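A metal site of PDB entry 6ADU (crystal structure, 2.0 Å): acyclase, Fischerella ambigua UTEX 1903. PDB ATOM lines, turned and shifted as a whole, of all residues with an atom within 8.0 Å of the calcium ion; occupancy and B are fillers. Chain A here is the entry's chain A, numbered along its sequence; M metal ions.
C of Ala 148 touches the calcium ion, at 3.9 Å. Six residues have an atom within 4 Å of the calcium ion: Asn 137, Leu 138, Phe 147, Ala 148, Gly 149 and Glu 175.
The backbone carbonyl oxygen of Asn 137 is in hydrogen-bond range of the backbone NH of Gly 176 (2.6 Å). The backbone carbonyl oxygen (O) of Gly 140 sits at hydrogen-bond distance from the backbone NH (N) of Phe 147, at 2.9 Å. N of Asn 137 lies within hydrogen-bond range of O of Glu 177 (3.0 Å). The backbone carbonyl oxygen of Ala 148 lies within hydrogen-bond range of the backbone NH of Phe 210 (2.9 Å). The side-chain amide nitrogen (ND2) of Asn 137 sits at hydrogen-bond distance from the backbone carbonyl oxygen (O) of Ile 173 (2.9 Å). OG of Ser 146 sits at hydrogen-bond distance from N of Ala 148 (3.3 Å).
The calcium ion is bound by O of Gly 149 (2.3 Å), O of Leu 138 (2.3 Å), OD1 of Asn 137 (2.4 Å), O of Phe 147 (2.4 Å) and OE1 of Glu 175 (2.7 Å). The calcium ion has five donor atoms within binding distance.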
ATOM      1  N   PHE A  88      -0.952  -2.559  -7.414  1.00  0.00           N
ATOM      2  CA  PHE A  88       0.373  -3.214  -7.319  1.00  0.00           C
ATOM      3  C   PHE A  88       0.869  -3.791  -8.650  1.00  0.00           C
ATOM      4  O   PHE A  88       2.070  -3.995  -8.762  1.00  0.00           O
ATOM      5  CB  PHE A  88       0.406  -4.339  -6.278  1.00  0.00           C
ATOM      6  CG  PHE A  88       0.292  -3.883  -4.836  1.00  0.00           C
ATOM      7  CD1 PHE A  88       1.129  -2.915  -4.335  1.00  0.00           C
ATOM      8  CD2 PHE A  88      -0.663  -4.437  -3.993  1.00  0.00           C
ATOM      9  CE1 PHE A  88       1.028  -2.500  -3.016  1.00  0.00           C
ATOM     10  CE2 PHE A  88      -0.764  -4.029  -2.686  1.00  0.00           C
ATOM     11  CZ  PHE A  88       0.068  -3.060  -2.193  1.00  0.00           C
ATOM     12  N   TYR A  89      -0.059  -4.101  -9.564  1.00  0.00           N
ATOM     13  CA  TYR A  89       0.194  -4.860 -10.769  1.00  0.00           C
ATOM     14  C   TYR A  89      -0.632  -4.285 -11.922  1.00  0.00           C
ATOM     15  O   TYR A  89      -1.667  -3.676 -11.685  1.00  0.00           O
ATOM     16  CB  TYR A  89      -0.168  -6.335 -10.565  1.00  0.00           C
ATOM     17  CG  TYR A  89       0.833  -7.072  -9.709  1.00  0.00           C
ATOM     18  CD1 TYR A  89       2.031  -7.525 -10.225  1.00  0.00           C
ATOM     19  CD2 TYR A  89       0.583  -7.298  -8.359  1.00  0.00           C
ATOM     20  CE1 TYR A  89       2.951  -8.189  -9.431  1.00  0.00           C
ATOM     21  CE2 TYR A  89       1.510  -7.913  -7.543  1.00  0.00           C
ATOM     22  CZ  TYR A  89       2.678  -8.386  -8.088  1.00  0.00           C
ATOM     23  OH  TYR A  89       3.564  -9.035  -7.292  1.00  0.00           O
ATOM     24  N   GLY A 136       6.057 -12.648  -9.117  1.00  0.00           N
ATOM     25  CA  GLY A 136       5.557 -11.300  -9.270  1.00  0.00           C
ATOM     26  C   GLY A 136       6.506 -10.292  -8.714  1.00  0.00           C
ATOM     27  O   GLY A 136       7.049 -10.508  -7.590  1.00  0.00           O
ATOM     28  N   ASN A 137       6.709  -9.224  -9.495  1.00  0.00           N
ATOM     29  CA  ASN A 137       7.453  -8.039  -9.169  1.00  0.00           C
ATOM     30  C   ASN A 137       6.451  -6.907  -8.917  1.00  0.00           C
ATOM     31  O   ASN A 137       5.831  -6.388  -9.876  1.00  0.00           O
ATOM     32  CB  ASN A 137       8.449  -7.694 -10.310  1.00  0.00           C
ATOM     33  CG  ASN A 137       9.315  -6.498  -9.986  1.00  0.00           C
ATOM     34  OD1 ASN A 137       9.154  -5.873  -8.953  1.00  0.00           O
ATOM     35  ND2 ASN A 137      10.289  -6.171 -10.850  1.00  0.00           N
ATOM     36  N   LEU A 138       6.285  -6.511  -7.650  1.00  0.00           N
ATOM     37  CA  LEU A 138       5.261  -5.544  -7.225  1.00  0.00           C
ATOM     38  C   LEU A 138       5.674  -4.138  -7.667  1.00  0.00           C
ATOM     39  O   LEU A 138       6.828  -3.812  -7.693  1.00  0.00           O
ATOM     40  CB  LEU A 138       5.203  -5.614  -5.701  1.00  0.00           C
ATOM     41  CG  LEU A 138       3.987  -5.000  -5.031  1.00  0.00           C
ATOM     42  CD1 LEU A 138       3.049  -6.100  -4.564  1.00  0.00           C
ATOM     43  CD2 LEU A 138       4.400  -4.140  -3.856  1.00  0.00           C
ATOM     44  N   ALA A 139       4.708  -3.316  -8.062  1.00  0.00           N
ATOM     45  CA  ALA A 139       5.043  -1.985  -8.574  1.00  0.00           C
ATOM     46  C   ALA A 139       4.307  -0.908  -7.773  1.00  0.00           C
ATOM     47  O   ALA A 139       3.324  -1.183  -7.101  1.00  0.00           O
ATOM     48  CB  ALA A 139       4.686  -1.930 -10.051  1.00  0.00           C
ATOM     49  N   GLY A 140       4.788   0.329  -7.873  1.00  0.00           N
ATOM     50  CA  GLY A 140       4.082   1.502  -7.354  1.00  0.00           C
ATOM     51  C   GLY A 140       4.745   2.131  -6.123  1.00  0.00           C
ATOM     52  O   GLY A 140       5.938   1.879  -5.795  1.00  0.00           O
ATOM     53  N   SER A 146       8.112   3.045  -1.373  1.00  0.00           N
ATOM     54  CA  SER A 146       8.415   2.719  -2.765  1.00  0.00           C
ATOM     55  C   SER A 146       8.539   1.206  -2.985  1.00  0.00           C
ATOM     56  O   SER A 146       9.324   0.575  -2.302  1.00  0.00           O
ATOM     57  CB  SER A 146       9.681   3.375  -3.213  1.00  0.00           C
ATOM     58  OG  SER A 146      10.052   2.820  -4.463  1.00  0.00           O
ATOM     59  N   PHE A 147       7.825   0.667  -3.965  1.00  0.00           N
ATOM     60  CA  PHE A 147       7.874  -0.751  -4.301  1.00  0.00           C
ATOM     61  C   PHE A 147       8.753  -1.026  -5.521  1.00  0.00           C
ATOM     62  O   PHE A 147       8.833  -2.160  -5.960  1.00  0.00           O
ATOM     63  CB  PHE A 147       6.467  -1.303  -4.505  1.00  0.00           C
ATOM     64  CG  PHE A 147       5.547  -0.913  -3.387  1.00  0.00           C
ATOM     65  CD1 PHE A 147       5.969  -1.010  -2.059  1.00  0.00           C
ATOM     66  CD2 PHE A 147       4.297  -0.371  -3.641  1.00  0.00           C
ATOM     67  CE1 PHE A 147       5.134  -0.613  -1.029  1.00  0.00           C
ATOM     68  CE2 PHE A 147       3.467   0.019  -2.615  1.00  0.00           C
ATOM     69  CZ  PHE A 147       3.883  -0.099  -1.308  1.00  0.00           C
ATOM     70  N   ALA A 148       9.510  -0.021  -5.994  1.00  0.00           N
ATOM     71  CA  ALA A 148      10.404  -0.248  -7.113  1.00  0.00           C
ATOM     72  C   ALA A 148      11.548  -1.159  -6.666  1.00  0.00           C
ATOM     73  O   ALA A 148      12.061  -1.056  -5.549  1.00  0.00           O
ATOM     74  CB  ALA A 148      10.934   1.059  -7.682  1.00  0.00           C
ATOM     75  N   GLY A 149      11.986  -2.002  -7.587  1.00  0.00           N
ATOM     76  CA  GLY A 149      13.066  -2.944  -7.380  1.00  0.00           C
ATOM     77  C   GLY A 149      12.507  -4.311  -7.027  1.00  0.00           C
ATOM     78  O   GLY A 149      11.296  -4.476  -6.830  1.00  0.00           O
ATOM     79  N   PHE A 150      13.412  -5.284  -6.878  1.00  0.00           N
ATOM     80  CA  PHE A 150      13.035  -6.706  -6.849  1.00  0.00           C
ATOM     81  C   PHE A 150      14.165  -7.444  -6.150  1.00  0.00           C
ATOM     82  O   PHE A 150      15.326  -7.107  -6.393  1.00  0.00           O
ATOM     83  CB  PHE A 150      12.831  -7.206  -8.281  1.00  0.00           C
ATOM     84  CG  PHE A 150      12.325  -8.639  -8.379  1.00  0.00           C
ATOM     85  CD1 PHE A 150      11.010  -8.931  -8.084  1.00  0.00           C
ATOM     86  CD2 PHE A 150      13.170  -9.667  -8.748  1.00  0.00           C
ATOM     87  CE1 PHE A 150      10.546 -10.237  -8.149  1.00  0.00           C
ATOM     88  CE2 PHE A 150      12.689 -10.966  -8.850  1.00  0.00           C
ATOM     89  CZ  PHE A 150      11.380 -11.251  -8.534  1.00  0.00           C
ATOM     90  N   PRO A 151      13.876  -8.378  -5.214  1.00  0.00           N
ATOM     91  CA  PRO A 151      14.923  -9.023  -4.426  1.00  0.00           C
ATOM     92  C   PRO A 151      15.592 -10.264  -5.019  1.00  0.00           C
ATOM     93  O   PRO A 151      16.584 -10.778  -4.449  1.00  0.00           O
ATOM     94  CB  PRO A 151      14.176  -9.473  -3.162  1.00  0.00           C
ATOM     95  CG  PRO A 151      12.784  -9.773  -3.669  1.00  0.00           C
ATOM     96  CD  PRO A 151      12.517  -8.749  -4.751  1.00  0.00           C
ATOM     97  N   ILE A 173      11.745 -10.020 -14.614  1.00  0.00           N
ATOM     98  CA  ILE A 173      10.353  -9.695 -14.369  1.00  0.00           C
ATOM     99  C   ILE A 173      10.186  -8.187 -14.217  1.00  0.00           C
ATOM    100  O   ILE A 173      10.784  -7.567 -13.335  1.00  0.00           O
ATOM    101  CB  ILE A 173       9.843 -10.453 -13.126  1.00  0.00           C
ATOM    102  CG1 ILE A 173      10.196 -11.943 -13.205  1.00  0.00           C
ATOM    103  CG2 ILE A 173       8.355 -10.216 -12.950  1.00  0.00           C
ATOM    104  CD1 ILE A 173       9.959 -12.671 -11.939  1.00  0.00           C
ATOM    105  N   LYS A 174       9.368  -7.602 -15.076  1.00  0.00           N
ATOM    106  CA  LYS A 174       9.093  -6.162 -15.045  1.00  0.00           C
ATOM    107  C   LYS A 174       8.256  -5.803 -13.815  1.00  0.00           C
ATOM    108  O   LYS A 174       7.451  -6.602 -13.326  1.00  0.00           O
ATOM    109  CB  LYS A 174       8.332  -5.728 -16.299  1.00  0.00           C
ATOM    110  CG  LYS A 174       9.110  -5.731 -17.612  1.00  0.00           C
ATOM    111  CD  LYS A 174       8.192  -5.457 -18.804  1.00  0.00           C
ATOM    112  CE  LYS A 174       7.726  -6.698 -19.538  1.00  0.00           C
ATOM    113  NZ  LYS A 174       8.374  -6.818 -20.869  1.00  0.00           N
ATOM    114  N   GLU A 175       8.444  -4.575 -13.373  1.00  0.00           N
ATOM    115  CA  GLU A 175       7.653  -3.953 -12.358  1.00  0.00           C
ATOM    116  C   GLU A 175       6.174  -4.112 -12.747  1.00  0.00           C
ATOM    117  O   GLU A 175       5.774  -3.722 -13.835  1.00  0.00           O
ATOM    118  CB  GLU A 175       8.045  -2.469 -12.260  1.00  0.00           C
ATOM    119  CG  GLU A 175       9.480  -2.225 -11.812  1.00  0.00           C
ATOM    120  CD  GLU A 175       9.761  -2.378 -10.318  1.00  0.00           C
ATOM    121  OE1 GLU A 175       8.781  -2.386  -9.503  1.00  0.00           O
ATOM    122  OE2 GLU A 175      10.934  -2.481  -9.958  1.00  0.00           O
ATOM    123  N   GLY A 176       5.391  -4.775 -11.897  1.00  0.00           N
ATOM    124  CA  GLY A 176       3.965  -4.853 -12.049  1.00  0.00           C
ATOM    125  C   GLY A 176       3.514  -6.000 -12.941  1.00  0.00           C
ATOM    126  O   GLY A 176       2.343  -6.030 -13.355  1.00  0.00           O
ATOM    127  N   GLU A 177       4.387  -6.988 -13.155  1.00  0.00           N
ATOM    128  CA  GLU A 177       4.014  -8.217 -13.858  1.00  0.00           C
ATOM    129  C   GLU A 177       4.421  -9.466 -13.060  1.00  0.00           C
ATOM    130  O   GLU A 177       5.265  -9.409 -12.091  1.00  0.00           O
ATOM    131  CB  GLU A 177       4.581  -8.242 -15.289  1.00  0.00           C
ATOM    132  CG  GLU A 177       6.031  -8.705 -15.394  1.00  0.00           C
ATOM    133  CD  GLU A 177       6.571  -8.985 -16.811  1.00  0.00           C
ATOM    134  OE1 GLU A 177       5.769  -9.405 -17.685  1.00  0.00           O
ATOM    135  OE2 GLU A 177       7.805  -8.785 -17.037  1.00  0.00           O
ATOM    136  N   LYS A 209      16.363  -4.345  -2.914  1.00  0.00           N
ATOM    137  CA  LYS A 209      15.137  -3.707  -2.460  1.00  0.00           C
ATOM    138  C   LYS A 209      14.484  -3.056  -3.677  1.00  0.00           C
ATOM    139  O   LYS A 209      15.186  -2.645  -4.611  1.00  0.00           O
ATOM    140  CB  LYS A 209      15.406  -2.623  -1.397  1.00  0.00           C
ATOM    141  CG  LYS A 209      16.281  -3.023  -0.214  1.00  0.00           C
ATOM    142  CD  LYS A 209      15.560  -3.135   1.128  1.00  0.00           C
ATOM    143  CE  LYS A 209      15.910  -4.369   1.944  1.00  0.00           C
ATOM    144  NZ  LYS A 209      14.780  -4.743   2.822  1.00  0.00           N
ATOM    145  N   PHE A 210      13.164  -2.926  -3.690  1.00  0.00           N
ATOM    146  CA  PHE A 210      12.227  -3.369  -2.658  1.00  0.00           C
ATOM    147  C   PHE A 210      12.214  -4.905  -2.577  1.00  0.00           C
ATOM    148  O   PHE A 210      12.281  -5.635  -3.606  1.00  0.00           O
ATOM    149  CB  PHE A 210      10.854  -2.802  -3.018  1.00  0.00           C
ATOM    150  CG  PHE A 210       9.656  -3.441  -2.371  1.00  0.00           C
ATOM    151  CD1 PHE A 210       9.247  -3.055  -1.122  1.00  0.00           C
ATOM    152  CD2 PHE A 210       8.925  -4.409  -3.037  1.00  0.00           C
ATOM    153  CE1 PHE A 210       8.137  -3.623  -0.525  1.00  0.00           C
ATOM    154  CE2 PHE A 210       7.814  -4.977  -2.440  1.00  0.00           C
ATOM    155  CZ  PHE A 210       7.423  -4.577  -1.192  1.00  0.00           C
ATOM    156  N   SER A 211      12.141  -5.423  -1.354  1.00  0.00           N
ATOM    157  CA  SER A 211      12.422  -6.839  -1.115  1.00  0.00           C
ATOM    158  C   SER A 211      11.159  -7.614  -0.697  1.00  0.00           C
ATOM    159  O   SER A 211      11.216  -8.483   0.160  1.00  0.00           O
ATOM    160  CB  SER A 211      13.574  -6.979  -0.143  1.00  0.00           C
ATOM    161  OG  SER A 211      13.366  -6.249   1.052  1.00  0.00           O
ATOM    162  N   GLY A 212      10.046  -7.288  -1.369  1.00  0.00           N
ATOM    163  CA  GLY A 212       8.846  -8.079  -1.446  1.00  0.00           C
ATOM    164  C   GLY A 212       8.807  -8.859  -2.759  1.00  0.00           C
ATOM    165  O   GLY A 212       9.317  -8.415  -3.786  1.00  0.00           O
ATOM    166  N   LEU A 213       8.251 -10.059  -2.702  1.00  0.00           N
ATOM    167  CA  LEU A 213       8.226 -11.027  -3.781  1.00  0.00           C
ATOM    168  C   LEU A 213       6.904 -11.783  -3.655  1.00  0.00           C
ATOM    169  O   LEU A 213       6.577 -12.168  -2.538  1.00  0.00           O
ATOM    170  CB  LEU A 213       9.426 -11.985  -3.602  1.00  0.00           C
ATOM    171  CG  LEU A 213       9.567 -13.076  -4.658  1.00  0.00           C
ATOM    172  CD1 LEU A 213       9.754 -12.438  -6.026  1.00  0.00           C
ATOM    173  CD2 LEU A 213      10.748 -13.992  -4.364  1.00  0.00           C
HETATM  174 CA    CA M   1       9.123  -4.075  -7.436  1.00  0.00          CA
